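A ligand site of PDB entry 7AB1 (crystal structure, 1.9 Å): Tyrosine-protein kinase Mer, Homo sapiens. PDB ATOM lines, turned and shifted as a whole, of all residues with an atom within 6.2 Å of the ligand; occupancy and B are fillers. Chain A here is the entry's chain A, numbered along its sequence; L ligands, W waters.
O of Leu 27 touches C14 of the ligand, 3.1 Å away.
CG2 of Val 35 touches N8 of the ligand, at 3.7 Å.
CB of Ala 51 touches C5 of the ligand, 3.3 Å away.
Ile 84 touches the ligand (CD1 to N3, 3.9 Å).
CB of Leu 105 touches N3 of the ligand, at 3.7 Å.
Phe 107 touches the ligand (C to O2, 3.6 Å).
Lys 109 touches the ligand (O to C23, 3.9 Å).
CA of Gly 111 touches C7 of the ligand (3.98 Å).
Asp 112 touches the ligand (OD1 to C20, 3.5 Å).
Tyr 119 touches the ligand.
CE of Met 164 touches C22 of the ligand, at 3.3 Å.
Ala 174 touches the ligand (CB to C1, 3.9 Å).
Asp 175 touches the ligand.
Hydrophobic or aromatic side chains within 4 Å of the ligand: Val 35, Ala 51, Ile 84, Leu 105, Phe 107, Met 108, Met 164 and Ala 174.
Of the 22 residues printed, 15 come within 4 Å of the ligand.
The nearest printed residue that does not touch the ligand is Arg 161 (4.2 Å).
O2 of the ligand lies within hydrogen-bond range of N of Met 108 (2.8 Å).
A nitrogen (N3) of the ligand is in hydrogen-bond range of the backbone carbonyl oxygen (O) of Pro 106 (2.9 Å).
Water W1 bridges OD1 of Asp 112 and O1 of the ligand.
N of Leu 27 sits at hydrogen-bond distance from O of Val 35, 2.8 Å away.
OD1 of Asp 175 lies within salt-bridge range of NZ of Lys 53.
The backbone NH of Val 35 sits at hydrogen-bond distance from the backbone carbonyl oxygen of Gly 28 (3.0 Å).
The side-chain carboxylate (OD1) of Asp 112 sits at hydrogen-bond distance from the side-chain hydroxyl (OG1) of Thr 115 (2.6 Å).
The backbone carbonyl oxygen of Asn 162 is in hydrogen-bond range of the backbone NH of Ala 174 (3.0 Å).
The backbone NH (N) of Ala 51 lies within hydrogen-bond range of the backbone carbonyl oxygen (O) of Leu 105, at 2.6 Å.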
ATOM      1  N   LEU A  27     -16.391 -22.045   8.328  1.00  0.00           N
ATOM      2  CA  LEU A  27     -15.596 -21.318   7.369  1.00  0.00           C
ATOM      3  C   LEU A  27     -14.218 -21.933   7.112  1.00  0.00           C
ATOM      4  O   LEU A  27     -13.535 -21.505   6.179  1.00  0.00           O
ATOM      5  CB  LEU A  27     -15.395 -19.897   7.877  1.00  0.00           C
ATOM      6  CG  LEU A  27     -16.644 -19.109   8.236  1.00  0.00           C
ATOM      7  CD1 LEU A  27     -16.259 -17.757   8.860  1.00  0.00           C
ATOM      8  CD2 LEU A  27     -17.521 -18.928   7.004  1.00  0.00           C
ATOM      9  N   GLY A  28     -13.794 -22.875   7.961  1.00  0.00           N
ATOM     10  CA  GLY A  28     -12.489 -23.526   7.804  1.00  0.00           C
ATOM     11  C   GLY A  28     -12.084 -24.315   9.040  1.00  0.00           C
ATOM     12  O   GLY A  28     -11.805 -23.722  10.079  1.00  0.00           O
ATOM     13  N   VAL A  35     -12.949 -22.193  12.427  1.00  0.00           N
ATOM     14  CA  VAL A  35     -13.537 -20.858  12.379  1.00  0.00           C
ATOM     15  C   VAL A  35     -14.899 -20.989  11.746  1.00  0.00           C
ATOM     16  O   VAL A  35     -15.042 -21.621  10.698  1.00  0.00           O
ATOM     17  CB  VAL A  35     -12.695 -19.879  11.554  1.00  0.00           C
ATOM     18  CG1 VAL A  35     -13.165 -18.465  11.801  1.00  0.00           C
ATOM     19  CG2 VAL A  35     -11.219 -20.021  11.913  1.00  0.00           C
ATOM     20  N   VAL A  50     -20.480 -12.188  13.175  1.00  0.00           N
ATOM     21  CA  VAL A  50     -19.138 -12.397  13.709  1.00  0.00           C
ATOM     22  C   VAL A  50     -18.499 -13.650  13.180  1.00  0.00           C
ATOM     23  O   VAL A  50     -19.150 -14.508  12.592  1.00  0.00           O
ATOM     24  CB  VAL A  50     -19.131 -12.445  15.272  1.00  0.00           C
ATOM     25  CG1 VAL A  50     -19.484 -11.114  15.802  1.00  0.00           C
ATOM     26  CG2 VAL A  50     -20.046 -13.535  15.792  1.00  0.00           C
ATOM     27  N   ALA A  51     -17.233 -13.762  13.457  1.00  0.00           N
ATOM     28  CA  ALA A  51     -16.500 -15.015  13.259  1.00  0.00           C
ATOM     29  C   ALA A  51     -16.244 -15.596  14.627  1.00  0.00           C
ATOM     30  O   ALA A  51     -16.083 -14.819  15.579  1.00  0.00           O
ATOM     31  CB  ALA A  51     -15.201 -14.720  12.588  1.00  0.00           C
ATOM     32  N   LYS A  53     -13.885 -18.600  16.589  1.00  0.00           N
ATOM     33  CA  LYS A  53     -12.735 -19.507  16.551  1.00  0.00           C
ATOM     34  C   LYS A  53     -12.802 -20.509  17.685  1.00  0.00           C
ATOM     35  O   LYS A  53     -12.858 -20.099  18.819  1.00  0.00           O
ATOM     36  CB  LYS A  53     -11.457 -18.687  16.666  1.00  0.00           C
ATOM     37  CG  LYS A  53     -10.236 -19.324  16.031  1.00  0.00           C
ATOM     38  CD  LYS A  53      -9.031 -18.388  16.026  1.00  0.00           C
ATOM     39  CE  LYS A  53      -8.381 -18.225  17.397  1.00  0.00           C
ATOM     40  NZ  LYS A  53      -7.464 -17.039  17.434  1.00  0.00           N
ATOM     41  N   ILE A  84      -6.816  -6.814  14.672  1.00  0.00           N
ATOM     42  CA  ILE A  84      -8.144  -7.408  14.731  1.00  0.00           C
ATOM     43  C   ILE A  84      -8.685  -7.330  16.164  1.00  0.00           C
ATOM     44  O   ILE A  84      -7.970  -7.662  17.117  1.00  0.00           O
ATOM     45  CB  ILE A  84      -8.140  -8.851  14.181  1.00  0.00           C
ATOM     46  CG1 ILE A  84      -9.555  -9.235  13.724  1.00  0.00           C
ATOM     47  CG2 ILE A  84      -7.604  -9.809  15.211  1.00  0.00           C
ATOM     48  CD1 ILE A  84      -9.662 -10.549  13.013  1.00  0.00           C
ATOM     49  N   LEU A 105     -14.720 -12.793  17.008  1.00  0.00           N
ATOM     50  CA  LEU A 105     -14.062 -11.795  16.219  1.00  0.00           C
ATOM     51  C   LEU A 105     -15.068 -11.182  15.240  1.00  0.00           C
ATOM     52  O   LEU A 105     -15.994 -11.853  14.800  1.00  0.00           O
ATOM     53  CB  LEU A 105     -12.965 -12.461  15.386  1.00  0.00           C
ATOM     54  CG  LEU A 105     -11.875 -13.153  16.171  1.00  0.00           C
ATOM     55  CD1 LEU A 105     -11.061 -14.028  15.226  1.00  0.00           C
ATOM     56  CD2 LEU A 105     -11.007 -12.093  16.826  1.00  0.00           C
ATOM     57  N   PRO A 106     -14.853  -9.923  14.854  1.00  0.00           N
ATOM     58  CA  PRO A 106     -15.619  -9.305  13.817  1.00  0.00           C
ATOM     59  C   PRO A 106     -15.423 -10.042  12.527  1.00  0.00           C
ATOM     60  O   PRO A 106     -14.326 -10.571  12.252  1.00  0.00           O
ATOM     61  CB  PRO A 106     -15.022  -7.896  13.707  1.00  0.00           C
ATOM     62  CG  PRO A 106     -13.806  -7.863  14.525  1.00  0.00           C
ATOM     63  CD  PRO A 106     -13.857  -9.015  15.452  1.00  0.00           C
ATOM     64  N   PHE A 107     -16.468 -10.105  11.721  1.00  0.00           N
ATOM     65  CA  PHE A 107     -16.413 -10.922  10.532  1.00  0.00           C
ATOM     66  C   PHE A 107     -15.491 -10.201   9.543  1.00  0.00           C
ATOM     67  O   PHE A 107     -15.464  -8.970   9.509  1.00  0.00           O
ATOM     68  CB  PHE A 107     -17.797 -11.151   9.989  1.00  0.00           C
ATOM     69  CG  PHE A 107     -17.861 -12.211   8.916  1.00  0.00           C
ATOM     70  CD1 PHE A 107     -17.680 -13.515   9.236  1.00  0.00           C
ATOM     71  CD2 PHE A 107     -18.076 -11.869   7.597  1.00  0.00           C
ATOM     72  CE1 PHE A 107     -17.718 -14.487   8.256  1.00  0.00           C
ATOM     73  CE2 PHE A 107     -18.115 -12.833   6.610  1.00  0.00           C
ATOM     74  CZ  PHE A 107     -17.946 -14.153   6.944  1.00  0.00           C
ATOM     75  N   MET A 108     -14.628 -10.946   8.835  1.00  0.00           N
ATOM     76  CA  MET A 108     -13.759 -10.312   7.830  1.00  0.00           C
ATOM     77  C   MET A 108     -14.223 -10.893   6.495  1.00  0.00           C
ATOM     78  O   MET A 108     -13.836 -11.995   6.120  1.00  0.00           O
ATOM     79  CB  MET A 108     -12.286 -10.578   8.101  1.00  0.00           C
ATOM     80  CG  MET A 108     -11.788 -10.083   9.458  1.00  0.00           C
ATOM     81  SD  MET A 108     -11.166  -8.414   9.464  1.00  0.00           S
ATOM     82  CE  MET A 108     -12.006  -7.757  10.911  1.00  0.00           C
ATOM     83  N   LYS A 109     -15.088 -10.134   5.808  1.00  0.00           N
ATOM     84  CA  LYS A 109     -15.768 -10.587   4.600  1.00  0.00           C
ATOM     85  C   LYS A 109     -14.843 -11.303   3.596  1.00  0.00           C
ATOM     86  O   LYS A 109     -15.193 -12.337   3.073  1.00  0.00           O
ATOM     87  CB  LYS A 109     -16.422  -9.375   3.911  1.00  0.00           C
ATOM     88  CG  LYS A 109     -17.423  -9.752   2.810  1.00  0.00           C
ATOM     89  CD  LYS A 109     -18.034  -8.526   2.147  1.00  0.00           C
ATOM     90  CE  LYS A 109     -18.983  -8.940   1.032  1.00  0.00           C
ATOM     91  NZ  LYS A 109     -19.586  -7.798   0.265  1.00  0.00           N
ATOM     92  N   TYR A 110     -13.652 -10.752   3.371  1.00  0.00           N
ATOM     93  CA  TYR A 110     -12.770 -11.222   2.311  1.00  0.00           C
ATOM     94  C   TYR A 110     -11.776 -12.285   2.735  1.00  0.00           C
ATOM     95  O   TYR A 110     -10.948 -12.687   1.900  1.00  0.00           O
ATOM     96  CB  TYR A 110     -12.077 -10.011   1.673  1.00  0.00           C
ATOM     97  CG  TYR A 110     -13.068  -9.157   0.923  1.00  0.00           C
ATOM     98  CD1 TYR A 110     -13.756  -9.678  -0.182  1.00  0.00           C
ATOM     99  CD2 TYR A 110     -13.344  -7.859   1.322  1.00  0.00           C
ATOM    100  CE1 TYR A 110     -14.691  -8.930  -0.861  1.00  0.00           C
ATOM    101  CE2 TYR A 110     -14.273  -7.092   0.635  1.00  0.00           C
ATOM    102  CZ  TYR A 110     -14.938  -7.639  -0.456  1.00  0.00           C
ATOM    103  OH  TYR A 110     -15.857  -6.917  -1.149  1.00  0.00           O
ATOM    104  N   GLY A 111     -11.847 -12.766   3.973  1.00  0.00           N
ATOM    105  CA  GLY A 111     -10.952 -13.811   4.454  1.00  0.00           C
ATOM    106  C   GLY A 111      -9.507 -13.317   4.616  1.00  0.00           C
ATOM    107  O   GLY A 111      -9.283 -12.097   4.761  1.00  0.00           O
ATOM    108  N   ASP A 112      -8.546 -14.254   4.592  1.00  0.00           N
ATOM    109  CA  ASP A 112      -7.128 -13.910   4.787  1.00  0.00           C
ATOM    110  C   ASP A 112      -6.478 -13.380   3.554  1.00  0.00           C
ATOM    111  O   ASP A 112      -6.822 -13.741   2.404  1.00  0.00           O
ATOM    112  CB  ASP A 112      -6.289 -15.103   5.260  1.00  0.00           C
ATOM    113  CG  ASP A 112      -6.032 -16.108   4.162  1.00  0.00           C
ATOM    114  OD1 ASP A 112      -7.019 -16.778   3.788  1.00  0.00           O
ATOM    115  OD2 ASP A 112      -4.863 -16.217   3.672  1.00  0.00           O
ATOM    116  N   THR A 115      -4.712 -16.052   0.767  1.00  0.00           N
ATOM    117  CA  THR A 115      -5.750 -16.569  -0.157  1.00  0.00           C
ATOM    118  C   THR A 115      -6.276 -15.521  -1.135  1.00  0.00           C
ATOM    119  O   THR A 115      -6.399 -15.765  -2.311  1.00  0.00           O
ATOM    120  CB  THR A 115      -6.908 -17.197   0.644  1.00  0.00           C
ATOM    121  OG1 THR A 115      -6.321 -18.069   1.614  1.00  0.00           O
ATOM    122  CG2 THR A 115      -7.787 -18.050  -0.273  1.00  0.00           C
ATOM    123  N   TYR A 119      -6.310 -15.714  -5.053  1.00  0.00           N
ATOM    124  CA  TYR A 119      -7.558 -15.645  -5.832  1.00  0.00           C
ATOM    125  C   TYR A 119      -7.500 -14.552  -6.868  1.00  0.00           C
ATOM    126  O   TYR A 119      -8.102 -14.663  -7.937  1.00  0.00           O
ATOM    127  CB  TYR A 119      -8.782 -15.378  -4.948  1.00  0.00           C
ATOM    128  CG  TYR A 119      -9.247 -16.503  -4.075  1.00  0.00           C
ATOM    129  CD1 TYR A 119      -9.232 -17.823  -4.508  1.00  0.00           C
ATOM    130  CD2 TYR A 119      -9.839 -16.218  -2.827  1.00  0.00           C
ATOM    131  CE1 TYR A 119      -9.726 -18.839  -3.708  1.00  0.00           C
ATOM    132  CE2 TYR A 119     -10.339 -17.230  -2.021  1.00  0.00           C
ATOM    133  CZ  TYR A 119     -10.276 -18.545  -2.467  1.00  0.00           C
ATOM    134  OH  TYR A 119     -10.756 -19.554  -1.674  1.00  0.00           O
ATOM    135  N   ARG A 161      -1.039 -15.107   5.594  1.00  0.00           N
ATOM    136  CA  ARG A 161      -2.197 -15.949   5.975  1.00  0.00           C
ATOM    137  C   ARG A 161      -2.869 -15.569   7.317  1.00  0.00           C
ATOM    138  O   ARG A 161      -4.013 -15.943   7.552  1.00  0.00           O
ATOM    139  CB  ARG A 161      -1.802 -17.422   5.993  1.00  0.00           C
ATOM    140  CG  ARG A 161      -0.828 -17.748   7.121  1.00  0.00           C
ATOM    141  CD  ARG A 161      -0.370 -19.185   7.174  1.00  0.00           C
ATOM    142  NE  ARG A 161       0.717 -19.317   8.162  1.00  0.00           N
ATOM    143  CZ  ARG A 161       2.013 -19.002   7.955  1.00  0.00           C
ATOM    144  NH1 ARG A 161       2.434 -18.540   6.772  1.00  0.00           N
ATOM    145  NH2 ARG A 161       2.911 -19.158   8.933  1.00  0.00           N
ATOM    146  N   ASN A 162      -2.134 -14.845   8.166  1.00  0.00           N
ATOM    147  CA  ASN A 162      -2.629 -14.232   9.421  1.00  0.00           C
ATOM    148  C   ASN A 162      -3.011 -12.761   9.385  1.00  0.00           C
ATOM    149  O   ASN A 162      -3.178 -12.145  10.440  1.00  0.00           O
ATOM    150  CB  ASN A 162      -1.553 -14.397  10.478  1.00  0.00           C
ATOM    151  CG  ASN A 162      -1.113 -15.843  10.626  1.00  0.00           C
ATOM    152  OD1 ASN A 162      -1.947 -16.742  10.536  1.00  0.00           O
ATOM    153  ND2 ASN A 162       0.172 -16.079  10.826  1.00  0.00           N
ATOM    154  N   MET A 164      -5.916 -10.209   7.833  1.00  0.00           N
ATOM    155  CA  MET A 164      -7.319 -10.398   7.436  1.00  0.00           C
ATOM    156  C   MET A 164      -7.798  -9.151   6.727  1.00  0.00           C
ATOM    157  O   MET A 164      -7.338  -8.046   7.023  1.00  0.00           O
ATOM    158  CB  MET A 164      -8.202 -10.687   8.622  1.00  0.00           C
ATOM    159  CG  MET A 164      -7.897 -11.958   9.378  1.00  0.00           C
ATOM    160  SD  MET A 164      -8.013 -13.481   8.416  1.00  0.00           S
ATOM    161  CE  MET A 164      -9.751 -13.468   8.056  1.00  0.00           C
ATOM    162  N   ALA A 174      -3.725 -10.305  12.735  1.00  0.00           N
ATOM    163  CA  ALA A 174      -4.491 -11.275  13.505  1.00  0.00           C
ATOM    164  C   ALA A 174      -3.605 -12.444  13.928  1.00  0.00           C
ATOM    165  O   ALA A 174      -2.386 -12.481  13.613  1.00  0.00           O
ATOM    166  CB  ALA A 174      -5.669 -11.779  12.663  1.00  0.00           C
ATOM    167  N   ASP A 175      -4.232 -13.367  14.677  1.00  0.00           N
ATOM    168  CA  ASP A 175      -3.623 -14.612  15.202  1.00  0.00           C
ATOM    169  C   ASP A 175      -2.275 -14.445  15.918  1.00  0.00           C
ATOM    170  O   ASP A 175      -1.342 -15.207  15.672  1.00  0.00           O
ATOM    171  CB  ASP A 175      -3.609 -15.690  14.119  1.00  0.00           C
ATOM    172  CG  ASP A 175      -5.016 -16.288  13.871  1.00  0.00           C
ATOM    173  OD1 ASP A 175      -5.872 -16.262  14.775  1.00  0.00           O
ATOM    174  OD2 ASP A 175      -5.286 -16.797  12.774  1.00  0.00           O
HETATM  175  C1  LIG L   1      -8.326 -14.570  12.545  1.00  0.00           C
HETATM  176  C2  LIG L   1      -9.014 -15.886  12.306  1.00  0.00           C
HETATM  177  C3  LIG L   1     -10.031 -15.824  11.191  1.00  0.00           C
HETATM  178  C4  LIG L   1     -11.894 -14.699  10.391  1.00  0.00           C
HETATM  179  C5  LIG L   1     -12.860 -13.567  10.639  1.00  0.00           C
HETATM  180  N1  LIG L   1     -12.983 -15.356   8.321  1.00  0.00           N
HETATM  181  C6  LIG L   1     -13.223 -15.877   7.033  1.00  0.00           C
HETATM  182  C7  LIG L   1     -14.189 -15.237   6.270  1.00  0.00           C
HETATM  183  C8  LIG L   1     -13.067 -17.050   2.166  1.00  0.00           C
HETATM  184  C9  LIG L   1     -13.634 -17.206   0.753  1.00  0.00           C
HETATM  185  C10 LIG L   1     -14.369 -18.540   0.616  1.00  0.00           C
HETATM  186  C11 LIG L   1     -15.432 -18.670   1.708  1.00  0.00           C
HETATM  187  C12 LIG L   1     -15.602 -20.647  -2.292  1.00  0.00           C
HETATM  188  C13 LIG L   1     -14.419 -18.114  -1.860  1.00  0.00           C
HETATM  189  O1  LIG L   1     -12.229 -18.482   4.630  1.00  0.00           O
HETATM  190  C14 LIG L   1     -11.475 -19.372   5.465  1.00  0.00           C
HETATM  191  C15 LIG L   1     -12.542 -16.975   6.505  1.00  0.00           C
HETATM  192  C16 LIG L   1     -10.107 -16.686  10.069  1.00  0.00           C
HETATM  193  C17 LIG L   1      -8.952 -18.376   8.634  1.00  0.00           C
HETATM  194  C18 LIG L   1      -8.840 -19.863   8.881  1.00  0.00           C
HETATM  195  C19 LIG L   1      -8.505 -20.551   7.587  1.00  0.00           C
HETATM  196  C20 LIG L   1      -7.421 -18.632   6.752  1.00  0.00           C
HETATM  197  C21 LIG L   1      -7.678 -17.845   8.013  1.00  0.00           C
HETATM  198  N2  LIG L   1     -10.942 -14.850  11.326  1.00  0.00           N
HETATM  199  O2  LIG L   1     -13.851 -13.390   9.911  1.00  0.00           O
HETATM  200  N3  LIG L   1     -12.591 -12.785  11.676  1.00  0.00           N
HETATM  201  C22 LIG L   1     -12.001 -15.530   9.259  1.00  0.00           C
HETATM  202  C23 LIG L   1     -14.483 -15.674   4.989  1.00  0.00           C
HETATM  203  C24 LIG L   1     -13.824 -16.761   4.460  1.00  0.00           C
HETATM  204  N4  LIG L   1     -14.110 -17.210   3.180  1.00  0.00           N
HETATM  205  C25 LIG L   1     -14.811 -18.491   3.082  1.00  0.00           C
HETATM  206  N5  LIG L   1     -14.938 -18.884  -0.720  1.00  0.00           N
HETATM  207  C26 LIG L   1     -14.843 -20.322  -1.021  1.00  0.00           C
HETATM  208  N6  LIG L   1     -15.083 -19.884  -3.425  1.00  0.00           N
HETATM  209  C27 LIG L   1     -15.813 -20.211  -4.655  1.00  0.00           C
HETATM  210  C28 LIG L   1     -15.178 -18.456  -3.134  1.00  0.00           C
HETATM  211  C29 LIG L   1     -12.843 -17.408   5.229  1.00  0.00           C
HETATM  212  N7  LIG L   1     -11.075 -16.509   9.148  1.00  0.00           N
HETATM  213  N8  LIG L   1      -9.225 -17.676   9.890  1.00  0.00           N
HETATM  214  O3  LIG L   1      -7.300 -20.026   7.009  1.00  0.00           O
HETATM  215  O   HOH W   1      -9.869 -16.749   3.214  1.00  0.00           O
